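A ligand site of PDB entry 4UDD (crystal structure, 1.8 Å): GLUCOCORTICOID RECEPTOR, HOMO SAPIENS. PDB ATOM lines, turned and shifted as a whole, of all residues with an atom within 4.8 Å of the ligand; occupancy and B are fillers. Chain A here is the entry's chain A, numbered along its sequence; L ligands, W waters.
OG1 of Thr 242 is in hydrogen-bond range of O4 of the ligand, 2.8 Å away. An oxygen (O5) of the ligand is in hydrogen-bond range of the guanidinium group (NH2) of Arg 114 (2.8 Å). The side-chain amide nitrogen (NE2) of Gln 73 sits at hydrogen-bond distance from an oxygen (O5) of the ligand, 3.1 Å away. An oxygen (O6) of the ligand is in hydrogen-bond range of the side-chain amide oxygen (OD1) of Asn 67 (3.1 Å).
The side-chain hydroxyl of Thr 242 sits at hydrogen-bond distance from the backbone carbonyl oxygen of Tyr 238. OG1 of Thr 242 sits at hydrogen-bond distance from O of Cys 239 (3.1 Å). The guanidinium group (NH2) of Arg 114 lies within hydrogen-bond range of the backbone carbonyl oxygen (O) of Phe 126. The side-chain sulfur of Met 107 lies within hydrogen-bond range of the side-chain amide nitrogen of Gln 73, 3.3 Å away. SD of Met 63 sits at hydrogen-bond distance from OH of Tyr 238 (3.6 Å). OE1 of Gln 145 is in hydrogen-bond range of OH of Tyr 238, at 2.6 Å. SG of Cys 146 lies within hydrogen-bond range of O of Met 142, at 3.4 Å.
CG of Met 63 touches C17 of the ligand, 3.5 Å away. O of Leu 66 touches C26 of the ligand, 3.5 Å away. Gly 70 touches the ligand. Met 104 touches the ligand (SD to C20, 3.8 Å). CB of Met 107 touches C22 of the ligand, at 3.8 Å. CD1 of Phe 126 touches C24 of the ligand (3.7 Å). Gln 145 touches the ligand (OE1 to C16, 3.9 Å). SG of Cys 146 touches C14 of the ligand, at 3.97 Å. CE of Met 149 touches C13 of the ligand, at 3.7 Å. CD1 of Tyr 238 touches O3 of the ligand, 3.2 Å away. Cys 239 touches the ligand. CG2 of Ile 250 touches O4 of the ligand (3.4 Å). CZ of Phe 252 touches O4 of the ligand (3.6 Å). Hydrophobic or aromatic side chains that line the ligand: Met 63, Leu 66, Met 104, Met 107, Phe 126, Met 149, Tyr 238, Ile 250 and Phe 252. Of the 27 residues printed, 17 come within 4 Å of the ligand. The nearest printed residue that does not touch the ligand is Ile 62 (4.02 Å).
Water W2 bridges O2 of the ligand (2.7 Å) and O of Gln 145 (2.7 Å). Water W1 lies within hydrogen-bond range of the backbone carbonyl oxygen of Met 107, the side-chain amide nitrogen of Gln 73, the guanidinium group of Arg 114 and an oxygen (O5) of the ligand.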
ATOM      1  N   THR A  59     -25.551  33.063  31.663  1.00  0.00           N
ATOM      2  CA  THR A  59     -24.899  32.268  30.630  1.00  0.00           C
ATOM      3  C   THR A  59     -25.272  30.801  30.809  1.00  0.00           C
ATOM      4  O   THR A  59     -25.588  30.149  29.825  1.00  0.00           O
ATOM      5  CB  THR A  59     -23.403  32.547  30.601  1.00  0.00           C
ATOM      6  OG1 THR A  59     -23.218  33.958  30.440  1.00  0.00           O
ATOM      7  CG2 THR A  59     -22.682  31.780  29.478  1.00  0.00           C
ATOM      8  N   ILE A  62     -28.771  30.039  29.461  1.00  0.00           N
ATOM      9  CA  ILE A  62     -28.743  30.098  27.987  1.00  0.00           C
ATOM     10  C   ILE A  62     -28.062  28.839  27.430  1.00  0.00           C
ATOM     11  O   ILE A  62     -28.612  28.211  26.522  1.00  0.00           O
ATOM     12  CB  ILE A  62     -28.069  31.422  27.503  1.00  0.00           C
ATOM     13  CG1 ILE A  62     -28.977  32.640  27.822  1.00  0.00           C
ATOM     14  CG2 ILE A  62     -27.740  31.371  25.975  1.00  0.00           C
ATOM     15  CD1 ILE A  62     -28.288  34.013  27.675  1.00  0.00           C
ATOM     16  N   MET A  63     -26.903  28.453  27.977  1.00  0.00           N
ATOM     17  CA  MET A  63     -26.182  27.252  27.511  1.00  0.00           C
ATOM     18  C   MET A  63     -27.067  26.011  27.643  1.00  0.00           C
ATOM     19  O   MET A  63     -27.171  25.220  26.691  1.00  0.00           O
ATOM     20  CB  MET A  63     -24.914  27.032  28.344  1.00  0.00           C
ATOM     21  CG  MET A  63     -23.829  28.024  28.076  1.00  0.00           C
ATOM     22  SD  MET A  63     -22.399  27.704  29.171  1.00  0.00           S
ATOM     23  CE  MET A  63     -23.067  27.886  30.597  1.00  0.00           C
ATOM     24  N   LEU A  66     -29.998  26.081  25.173  1.00  0.00           N
ATOM     25  CA  LEU A  66     -29.496  25.804  23.821  1.00  0.00           C
ATOM     26  C   LEU A  66     -29.180  24.347  23.609  1.00  0.00           C
ATOM     27  O   LEU A  66     -29.501  23.823  22.545  1.00  0.00           O
ATOM     28  CB  LEU A  66     -28.324  26.713  23.467  1.00  0.00           C
ATOM     29  CG  LEU A  66     -28.680  28.195  23.309  1.00  0.00           C
ATOM     30  CD1 LEU A  66     -27.433  29.014  22.998  1.00  0.00           C
ATOM     31  CD2 LEU A  66     -29.744  28.388  22.214  1.00  0.00           C
ATOM     32  N   ASN A  67     -28.607  23.643  24.621  1.00  0.00           N
ATOM     33  CA  ASN A  67     -28.382  22.196  24.486  1.00  0.00           C
ATOM     34  C   ASN A  67     -29.707  21.478  24.291  1.00  0.00           C
ATOM     35  O   ASN A  67     -29.816  20.610  23.416  1.00  0.00           O
ATOM     36  CB  ASN A  67     -27.629  21.646  25.701  1.00  0.00           C
ATOM     37  CG  ASN A  67     -26.196  22.104  25.727  1.00  0.00           C
ATOM     38  OD1 ASN A  67     -25.630  22.442  24.683  1.00  0.00           O
ATOM     39  ND2 ASN A  67     -25.555  22.066  26.874  1.00  0.00           N
ATOM     40  N   LEU A  69     -32.519  22.726  23.007  1.00  0.00           N
ATOM     41  CA  LEU A  69     -32.934  23.091  21.645  1.00  0.00           C
ATOM     42  C   LEU A  69     -32.160  22.259  20.598  1.00  0.00           C
ATOM     43  O   LEU A  69     -32.756  21.728  19.672  1.00  0.00           O
ATOM     44  CB  LEU A  69     -32.696  24.596  21.424  1.00  0.00           C
ATOM     45  CG  LEU A  69     -33.013  25.171  20.018  1.00  0.00           C
ATOM     46  CD1 LEU A  69     -34.511  25.023  19.687  1.00  0.00           C
ATOM     47  CD2 LEU A  69     -32.596  26.615  19.930  1.00  0.00           C
ATOM     48  N   GLY A  70     -30.838  22.161  20.785  1.00  0.00           N
ATOM     49  CA  GLY A  70     -29.946  21.413  19.902  1.00  0.00           C
ATOM     50  C   GLY A  70     -30.344  19.959  19.755  1.00  0.00           C
ATOM     51  O   GLY A  70     -30.262  19.415  18.658  1.00  0.00           O
ATOM     52  N   GLN A  73     -33.368  19.902  17.508  1.00  0.00           N
ATOM     53  CA  GLN A  73     -32.939  20.220  16.146  1.00  0.00           C
ATOM     54  C   GLN A  73     -32.253  18.990  15.520  1.00  0.00           C
ATOM     55  O   GLN A  73     -32.437  18.737  14.344  1.00  0.00           O
ATOM     56  CB  GLN A  73     -31.987  21.416  16.143  1.00  0.00           C
ATOM     57  CG  GLN A  73     -32.710  22.746  16.307  1.00  0.00           C
ATOM     58  CD  GLN A  73     -31.764  23.911  16.360  1.00  0.00           C
ATOM     59  OE1 GLN A  73     -32.167  25.052  16.527  1.00  0.00           O
ATOM     60  NE2 GLN A  73     -30.482  23.665  16.171  1.00  0.00           N
ATOM     61  N   TRP A 103     -23.095  16.703  12.597  1.00  0.00           N
ATOM     62  CA  TRP A 103     -24.118  17.334  13.421  1.00  0.00           C
ATOM     63  C   TRP A 103     -23.818  18.821  13.778  1.00  0.00           C
ATOM     64  O   TRP A 103     -24.695  19.673  13.566  1.00  0.00           O
ATOM     65  CB  TRP A 103     -24.407  16.496  14.681  1.00  0.00           C
ATOM     66  CG  TRP A 103     -23.486  16.717  15.847  1.00  0.00           C
ATOM     67  CD1 TRP A 103     -22.260  16.160  16.043  1.00  0.00           C
ATOM     68  CD2 TRP A 103     -23.730  17.593  16.964  1.00  0.00           C
ATOM     69  NE1 TRP A 103     -21.722  16.603  17.235  1.00  0.00           N
ATOM     70  CE2 TRP A 103     -22.608  17.483  17.822  1.00  0.00           C
ATOM     71  CE3 TRP A 103     -24.760  18.485  17.305  1.00  0.00           C
ATOM     72  CZ2 TRP A 103     -22.513  18.204  19.016  1.00  0.00           C
ATOM     73  CZ3 TRP A 103     -24.657  19.205  18.493  1.00  0.00           C
ATOM     74  CH2 TRP A 103     -23.555  19.051  19.336  1.00  0.00           C
ATOM     75  N   MET A 104     -22.609  19.142  14.294  1.00  0.00           N
ATOM     76  CA  MET A 104     -22.277  20.524  14.684  1.00  0.00           C
ATOM     77  C   MET A 104     -22.217  21.464  13.478  1.00  0.00           C
ATOM     78  O   MET A 104     -22.616  22.636  13.590  1.00  0.00           O
ATOM     79  CB  MET A 104     -20.986  20.609  15.514  1.00  0.00           C
ATOM     80  CG  MET A 104     -20.696  22.021  16.085  1.00  0.00           C
ATOM     81  SD  MET A 104     -21.948  22.636  17.279  1.00  0.00           S
ATOM     82  CE  MET A 104     -21.395  21.829  18.754  1.00  0.00           C
ATOM     83  N   MET A 107     -25.868  22.320  12.473  1.00  0.00           N
ATOM     84  CA  MET A 107     -26.483  23.254  13.423  1.00  0.00           C
ATOM     85  C   MET A 107     -25.929  24.636  13.296  1.00  0.00           C
ATOM     86  O   MET A 107     -26.702  25.603  13.314  1.00  0.00           O
ATOM     87  CB  MET A 107     -26.326  22.796  14.896  1.00  0.00           C
ATOM     88  CG  MET A 107     -26.715  21.383  15.151  1.00  0.00           C
ATOM     89  SD  MET A 107     -28.475  21.162  15.278  1.00  0.00           S
ATOM     90  CE  MET A 107     -28.884  20.780  13.651  1.00  0.00           C
ATOM     91  N   ALA A 108     -24.583  24.758  13.222  1.00  0.00           N
ATOM     92  CA  ALA A 108     -23.926  26.055  13.109  1.00  0.00           C
ATOM     93  C   ALA A 108     -24.246  26.710  11.760  1.00  0.00           C
ATOM     94  O   ALA A 108     -24.456  27.931  11.698  1.00  0.00           O
ATOM     95  CB  ALA A 108     -22.427  25.924  13.295  1.00  0.00           C
ATOM     96  N   LEU A 111     -27.876  27.825  11.880  1.00  0.00           N
ATOM     97  CA  LEU A 111     -27.856  28.977  12.769  1.00  0.00           C
ATOM     98  C   LEU A 111     -27.373  30.224  12.005  1.00  0.00           C
ATOM     99  O   LEU A 111     -27.979  31.290  12.135  1.00  0.00           O
ATOM    100  CB  LEU A 111     -26.945  28.731  14.002  1.00  0.00           C
ATOM    101  CG  LEU A 111     -26.604  29.962  14.806  1.00  0.00           C
ATOM    102  CD1 LEU A 111     -27.836  30.517  15.529  1.00  0.00           C
ATOM    103  CD2 LEU A 111     -25.528  29.631  15.803  1.00  0.00           C
ATOM    104  N   ARG A 114     -30.291  31.443   9.765  1.00  0.00           N
ATOM    105  CA  ARG A 114     -31.344  32.132  10.522  1.00  0.00           C
ATOM    106  C   ARG A 114     -30.884  33.502  10.985  1.00  0.00           C
ATOM    107  O   ARG A 114     -31.657  34.448  10.878  1.00  0.00           O
ATOM    108  CB  ARG A 114     -31.840  31.305  11.715  1.00  0.00           C
ATOM    109  CG  ARG A 114     -32.500  29.980  11.316  1.00  0.00           C
ATOM    110  CD  ARG A 114     -33.171  29.284  12.487  1.00  0.00           C
ATOM    111  NE  ARG A 114     -32.276  29.084  13.640  1.00  0.00           N
ATOM    112  CZ  ARG A 114     -31.449  28.045  13.785  1.00  0.00           C
ATOM    113  NH1 ARG A 114     -31.358  27.131  12.832  1.00  0.00           N
ATOM    114  NH2 ARG A 114     -30.714  27.931  14.880  1.00  0.00           N
ATOM    115  N   PHE A 126     -30.642  31.953  17.529  1.00  0.00           N
ATOM    116  CA  PHE A 126     -30.768  30.516  17.824  1.00  0.00           C
ATOM    117  C   PHE A 126     -32.194  30.018  17.626  1.00  0.00           C
ATOM    118  O   PHE A 126     -32.404  28.933  17.105  1.00  0.00           O
ATOM    119  CB  PHE A 126     -30.299  30.217  19.261  1.00  0.00           C
ATOM    120  CG  PHE A 126     -28.793  30.293  19.410  1.00  0.00           C
ATOM    121  CD1 PHE A 126     -27.984  29.220  19.015  1.00  0.00           C
ATOM    122  CD2 PHE A 126     -28.188  31.403  19.983  1.00  0.00           C
ATOM    123  CE1 PHE A 126     -26.598  29.281  19.160  1.00  0.00           C
ATOM    124  CE2 PHE A 126     -26.795  31.463  20.122  1.00  0.00           C
ATOM    125  CZ  PHE A 126     -26.014  30.399  19.725  1.00  0.00           C
ATOM    126  N   ILE A 132     -29.193  36.347  20.714  1.00  0.00           N
ATOM    127  CA  ILE A 132     -28.135  36.965  21.509  1.00  0.00           C
ATOM    128  C   ILE A 132     -28.068  38.444  21.121  1.00  0.00           C
ATOM    129  O   ILE A 132     -27.263  38.858  20.279  1.00  0.00           O
ATOM    130  CB  ILE A 132     -26.769  36.206  21.446  1.00  0.00           C
ATOM    131  CG1 ILE A 132     -26.927  34.686  21.733  1.00  0.00           C
ATOM    132  CG2 ILE A 132     -25.710  36.846  22.366  1.00  0.00           C
ATOM    133  CD1 ILE A 132     -27.670  34.224  23.043  1.00  0.00           C
ATOM    134  N   MET A 142     -18.888  37.103  26.223  1.00  0.00           N
ATOM    135  CA  MET A 142     -19.898  36.662  25.268  1.00  0.00           C
ATOM    136  C   MET A 142     -19.447  36.771  23.812  1.00  0.00           C
ATOM    137  O   MET A 142     -19.678  35.829  23.066  1.00  0.00           O
ATOM    138  CB  MET A 142     -21.240  37.388  25.487  1.00  0.00           C
ATOM    139  CG  MET A 142     -22.444  36.721  24.795  1.00  0.00           C
ATOM    140  SD  MET A 142     -22.543  34.906  24.897  1.00  0.00           S
ATOM    141  CE  MET A 142     -22.888  34.692  26.658  1.00  0.00           C
ATOM    142  N   GLN A 145     -17.300  33.921  22.821  1.00  0.00           N
ATOM    143  CA  GLN A 145     -18.116  32.702  22.777  1.00  0.00           C
ATOM    144  C   GLN A 145     -18.989  32.658  21.509  1.00  0.00           C
ATOM    145  O   GLN A 145     -19.431  31.575  21.110  1.00  0.00           O
ATOM    146  CB  GLN A 145     -19.044  32.625  24.005  1.00  0.00           C
ATOM    147  CG  GLN A 145     -18.313  32.472  25.345  1.00  0.00           C
ATOM    148  CD  GLN A 145     -19.299  32.406  26.470  1.00  0.00           C
ATOM    149  OE1 GLN A 145     -20.148  31.517  26.519  1.00  0.00           O
ATOM    150  NE2 GLN A 145     -19.214  33.351  27.382  1.00  0.00           N
ATOM    151  N   CYS A 146     -19.258  33.821  20.897  1.00  0.00           N
ATOM    152  CA  CYS A 146     -20.142  33.928  19.738  1.00  0.00           C
ATOM    153  C   CYS A 146     -19.461  34.156  18.383  1.00  0.00           C
ATOM    154  O   CYS A 146     -20.092  33.940  17.352  1.00  0.00           O
ATOM    155  CB  CYS A 146     -21.180  35.017  19.987  1.00  0.00           C
ATOM    156  SG  CYS A 146     -22.336  34.648  21.338  1.00  0.00           S
ATOM    157  N   MET A 149     -19.476  31.516  15.378  1.00  0.00           N
ATOM    158  CA  MET A 149     -20.842  31.387  14.835  1.00  0.00           C
ATOM    159  C   MET A 149     -21.272  32.664  14.103  1.00  0.00           C
ATOM    160  O   MET A 149     -21.893  32.565  13.037  1.00  0.00           O
ATOM    161  CB  MET A 149     -21.837  31.009  15.922  1.00  0.00           C
ATOM    162  CG  MET A 149     -21.672  29.584  16.394  1.00  0.00           C
ATOM    163  SD  MET A 149     -22.656  29.170  17.853  1.00  0.00           S
ATOM    164  CE  MET A 149     -21.750  29.997  19.121  1.00  0.00           C
ATOM    165  N   LEU A 235     -16.242  25.116  18.006  1.00  0.00           N
ATOM    166  CA  LEU A 235     -17.506  24.808  18.687  1.00  0.00           C
ATOM    167  C   LEU A 235     -17.470  23.489  19.441  1.00  0.00           C
ATOM    168  O   LEU A 235     -17.995  23.407  20.548  1.00  0.00           O
ATOM    169  CB  LEU A 235     -18.711  24.856  17.725  1.00  0.00           C
ATOM    170  CG  LEU A 235     -18.918  26.191  16.983  1.00  0.00           C
ATOM    171  CD1 LEU A 235     -20.089  26.078  16.021  1.00  0.00           C
ATOM    172  CD2 LEU A 235     -19.103  27.361  17.963  1.00  0.00           C
ATOM    173  N   TYR A 238     -15.547  23.725  22.792  1.00  0.00           N
ATOM    174  CA  TYR A 238     -16.438  24.275  23.818  1.00  0.00           C
ATOM    175  C   TYR A 238     -17.453  23.185  24.268  1.00  0.00           C
ATOM    176  O   TYR A 238     -17.574  22.902  25.466  1.00  0.00           O
ATOM    177  CB  TYR A 238     -17.163  25.518  23.250  1.00  0.00           C
ATOM    178  CG  TYR A 238     -17.826  26.421  24.270  1.00  0.00           C
ATOM    179  CD1 TYR A 238     -18.711  25.911  25.215  1.00  0.00           C
ATOM    180  CD2 TYR A 238     -17.725  27.808  24.157  1.00  0.00           C
ATOM    181  CE1 TYR A 238     -19.366  26.742  26.111  1.00  0.00           C
ATOM    182  CE2 TYR A 238     -18.408  28.655  25.036  1.00  0.00           C
ATOM    183  CZ  TYR A 238     -19.221  28.113  26.015  1.00  0.00           C
ATOM    184  OH  TYR A 238     -19.917  28.908  26.889  1.00  0.00           O
ATOM    185  N   CYS A 239     -18.139  22.583  23.305  1.00  0.00           N
ATOM    186  CA  CYS A 239     -19.122  21.538  23.539  1.00  0.00           C
ATOM    187  C   CYS A 239     -18.533  20.374  24.359  1.00  0.00           C
ATOM    188  O   CYS A 239     -19.125  19.978  25.370  1.00  0.00           O
ATOM    189  CB  CYS A 239     -19.695  21.050  22.218  1.00  0.00           C
ATOM    190  SG  CYS A 239     -20.879  19.692  22.393  1.00  0.00           S
ATOM    191  N   THR A 242     -17.676  21.350  28.063  1.00  0.00           N
ATOM    192  CA  THR A 242     -18.877  21.479  28.904  1.00  0.00           C
ATOM    193  C   THR A 242     -19.574  20.146  29.109  1.00  0.00           C
ATOM    194  O   THR A 242     -20.245  19.962  30.126  1.00  0.00           O
ATOM    195  CB  THR A 242     -19.837  22.580  28.390  1.00  0.00           C
ATOM    196  OG1 THR A 242     -20.330  22.244  27.100  1.00  0.00           O
ATOM    197  CG2 THR A 242     -19.169  23.961  28.349  1.00  0.00           C
ATOM    198  N   ILE A 250     -23.628  21.396  33.412  1.00  0.00           N
ATOM    199  CA  ILE A 250     -24.210  21.723  32.100  1.00  0.00           C
ATOM    200  C   ILE A 250     -24.795  20.439  31.514  1.00  0.00           C
ATOM    201  O   ILE A 250     -24.062  19.515  31.179  1.00  0.00           O
ATOM    202  CB  ILE A 250     -23.242  22.454  31.123  1.00  0.00           C
ATOM    203  CG1 ILE A 250     -22.895  23.864  31.666  1.00  0.00           C
ATOM    204  CG2 ILE A 250     -23.872  22.528  29.712  1.00  0.00           C
ATOM    205  CD1 ILE A 250     -21.648  24.428  31.121  1.00  0.00           C
ATOM    206  N   PHE A 252     -26.977  18.074  28.830  1.00  0.00           N
ATOM    207  CA  PHE A 252     -27.184  17.828  27.416  1.00  0.00           C
ATOM    208  C   PHE A 252     -28.321  16.821  27.321  1.00  0.00           C
ATOM    209  O   PHE A 252     -28.348  15.860  28.106  1.00  0.00           O
ATOM    210  CB  PHE A 252     -25.935  17.235  26.757  1.00  0.00           C
ATOM    211  CG  PHE A 252     -24.844  18.238  26.494  1.00  0.00           C
ATOM    212  CD1 PHE A 252     -23.995  18.655  27.518  1.00  0.00           C
ATOM    213  CD2 PHE A 252     -24.693  18.816  25.230  1.00  0.00           C
ATOM    214  CE1 PHE A 252     -23.015  19.617  27.276  1.00  0.00           C
ATOM    215  CE2 PHE A 252     -23.698  19.759  24.991  1.00  0.00           C
ATOM    216  CZ  PHE A 252     -22.855  20.147  26.028  1.00  0.00           C
ATOM    217  N   LEU A 256     -28.044  14.565  22.023  1.00  0.00           N
ATOM    218  CA  LEU A 256     -26.707  15.125  21.951  1.00  0.00           C
ATOM    219  C   LEU A 256     -25.679  14.325  22.721  1.00  0.00           C
ATOM    220  O   LEU A 256     -24.579  14.128  22.216  1.00  0.00           O
ATOM    221  CB  LEU A 256     -26.676  16.613  22.380  1.00  0.00           C
ATOM    222  CG  LEU A 256     -27.507  17.592  21.543  1.00  0.00           C
ATOM    223  CD1 LEU A 256     -27.115  19.056  21.868  1.00  0.00           C
ATOM    224  CD2 LEU A 256     -27.339  17.333  20.023  1.00  0.00           C
HETATM  225  C1  LIG L   1     -23.144  23.161  22.300  1.00  0.00           C
HETATM  226  C2  LIG L   1     -23.499  24.682  22.364  1.00  0.00           C
HETATM  227  C3  LIG L   1     -24.983  24.889  22.725  1.00  0.00           C
HETATM  228  C4  LIG L   1     -25.936  24.404  21.620  1.00  0.00           C
HETATM  229  C5  LIG L   1     -25.630  24.970  20.200  1.00  0.00           C
HETATM  230  C6  LIG L   1     -24.107  24.844  19.825  1.00  0.00           C
HETATM  231  C7  LIG L   1     -23.249  25.418  20.994  1.00  0.00           C
HETATM  232  C8  LIG L   1     -21.710  25.487  20.922  1.00  0.00           C
HETATM  233  C9  LIG L   1     -21.308  25.851  22.386  1.00  0.00           C
HETATM  234  C10 LIG L   1     -22.523  25.444  23.299  1.00  0.00           C
HETATM  235  O1  LIG L   1     -23.100  26.718  23.688  1.00  0.00           O
HETATM  236  C11 LIG L   1     -22.004  27.649  23.652  1.00  0.00           C
HETATM  237  O2  LIG L   1     -21.264  27.289  22.465  1.00  0.00           O
HETATM  238  C12 LIG L   1     -22.478  29.106  23.664  1.00  0.00           C
HETATM  239  C13 LIG L   1     -23.282  29.518  22.430  1.00  0.00           C
HETATM  240  C14 LIG L   1     -23.532  31.044  22.501  1.00  0.00           C
HETATM  241  C15 LIG L   1     -24.397  31.348  23.741  1.00  0.00           C
HETATM  242  C16 LIG L   1     -23.654  30.900  25.017  1.00  0.00           C
HETATM  243  C17 LIG L   1     -23.292  29.398  24.942  1.00  0.00           C
HETATM  244  C18 LIG L   1     -22.150  24.649  24.536  1.00  0.00           C
HETATM  245  O3  LIG L   1     -21.174  23.933  24.516  1.00  0.00           O
HETATM  246  C19 LIG L   1     -22.992  24.744  25.798  1.00  0.00           C
HETATM  247  O4  LIG L   1     -22.696  23.688  26.722  1.00  0.00           O
HETATM  248  C20 LIG L   1     -23.838  25.665  18.532  1.00  0.00           C
HETATM  249  C21 LIG L   1     -24.751  25.243  17.373  1.00  0.00           C
HETATM  250  C22 LIG L   1     -26.217  25.173  17.832  1.00  0.00           C
HETATM  251  C23 LIG L   1     -27.111  25.823  17.103  1.00  0.00           C
HETATM  252  C24 LIG L   1     -28.531  25.839  17.525  1.00  0.00           C
HETATM  253  O5  LIG L   1     -29.365  26.425  16.879  1.00  0.00           O
HETATM  254  C25 LIG L   1     -28.925  25.148  18.774  1.00  0.00           C
HETATM  255  C26 LIG L   1     -28.017  24.494  19.475  1.00  0.00           C
HETATM  256  C27 LIG L   1     -26.551  24.390  19.068  1.00  0.00           C
HETATM  257  C28 LIG L   1     -26.362  22.884  18.721  1.00  0.00           C
HETATM  258  O6  LIG L   1     -26.058  22.979  21.690  1.00  0.00           O
HETATM  259  O   HOH W   1     -29.369  25.171  14.069  1.00  0.00           O
HETATM  260  O   HOH W   2     -19.288  28.854  21.435  1.00  0.00           O
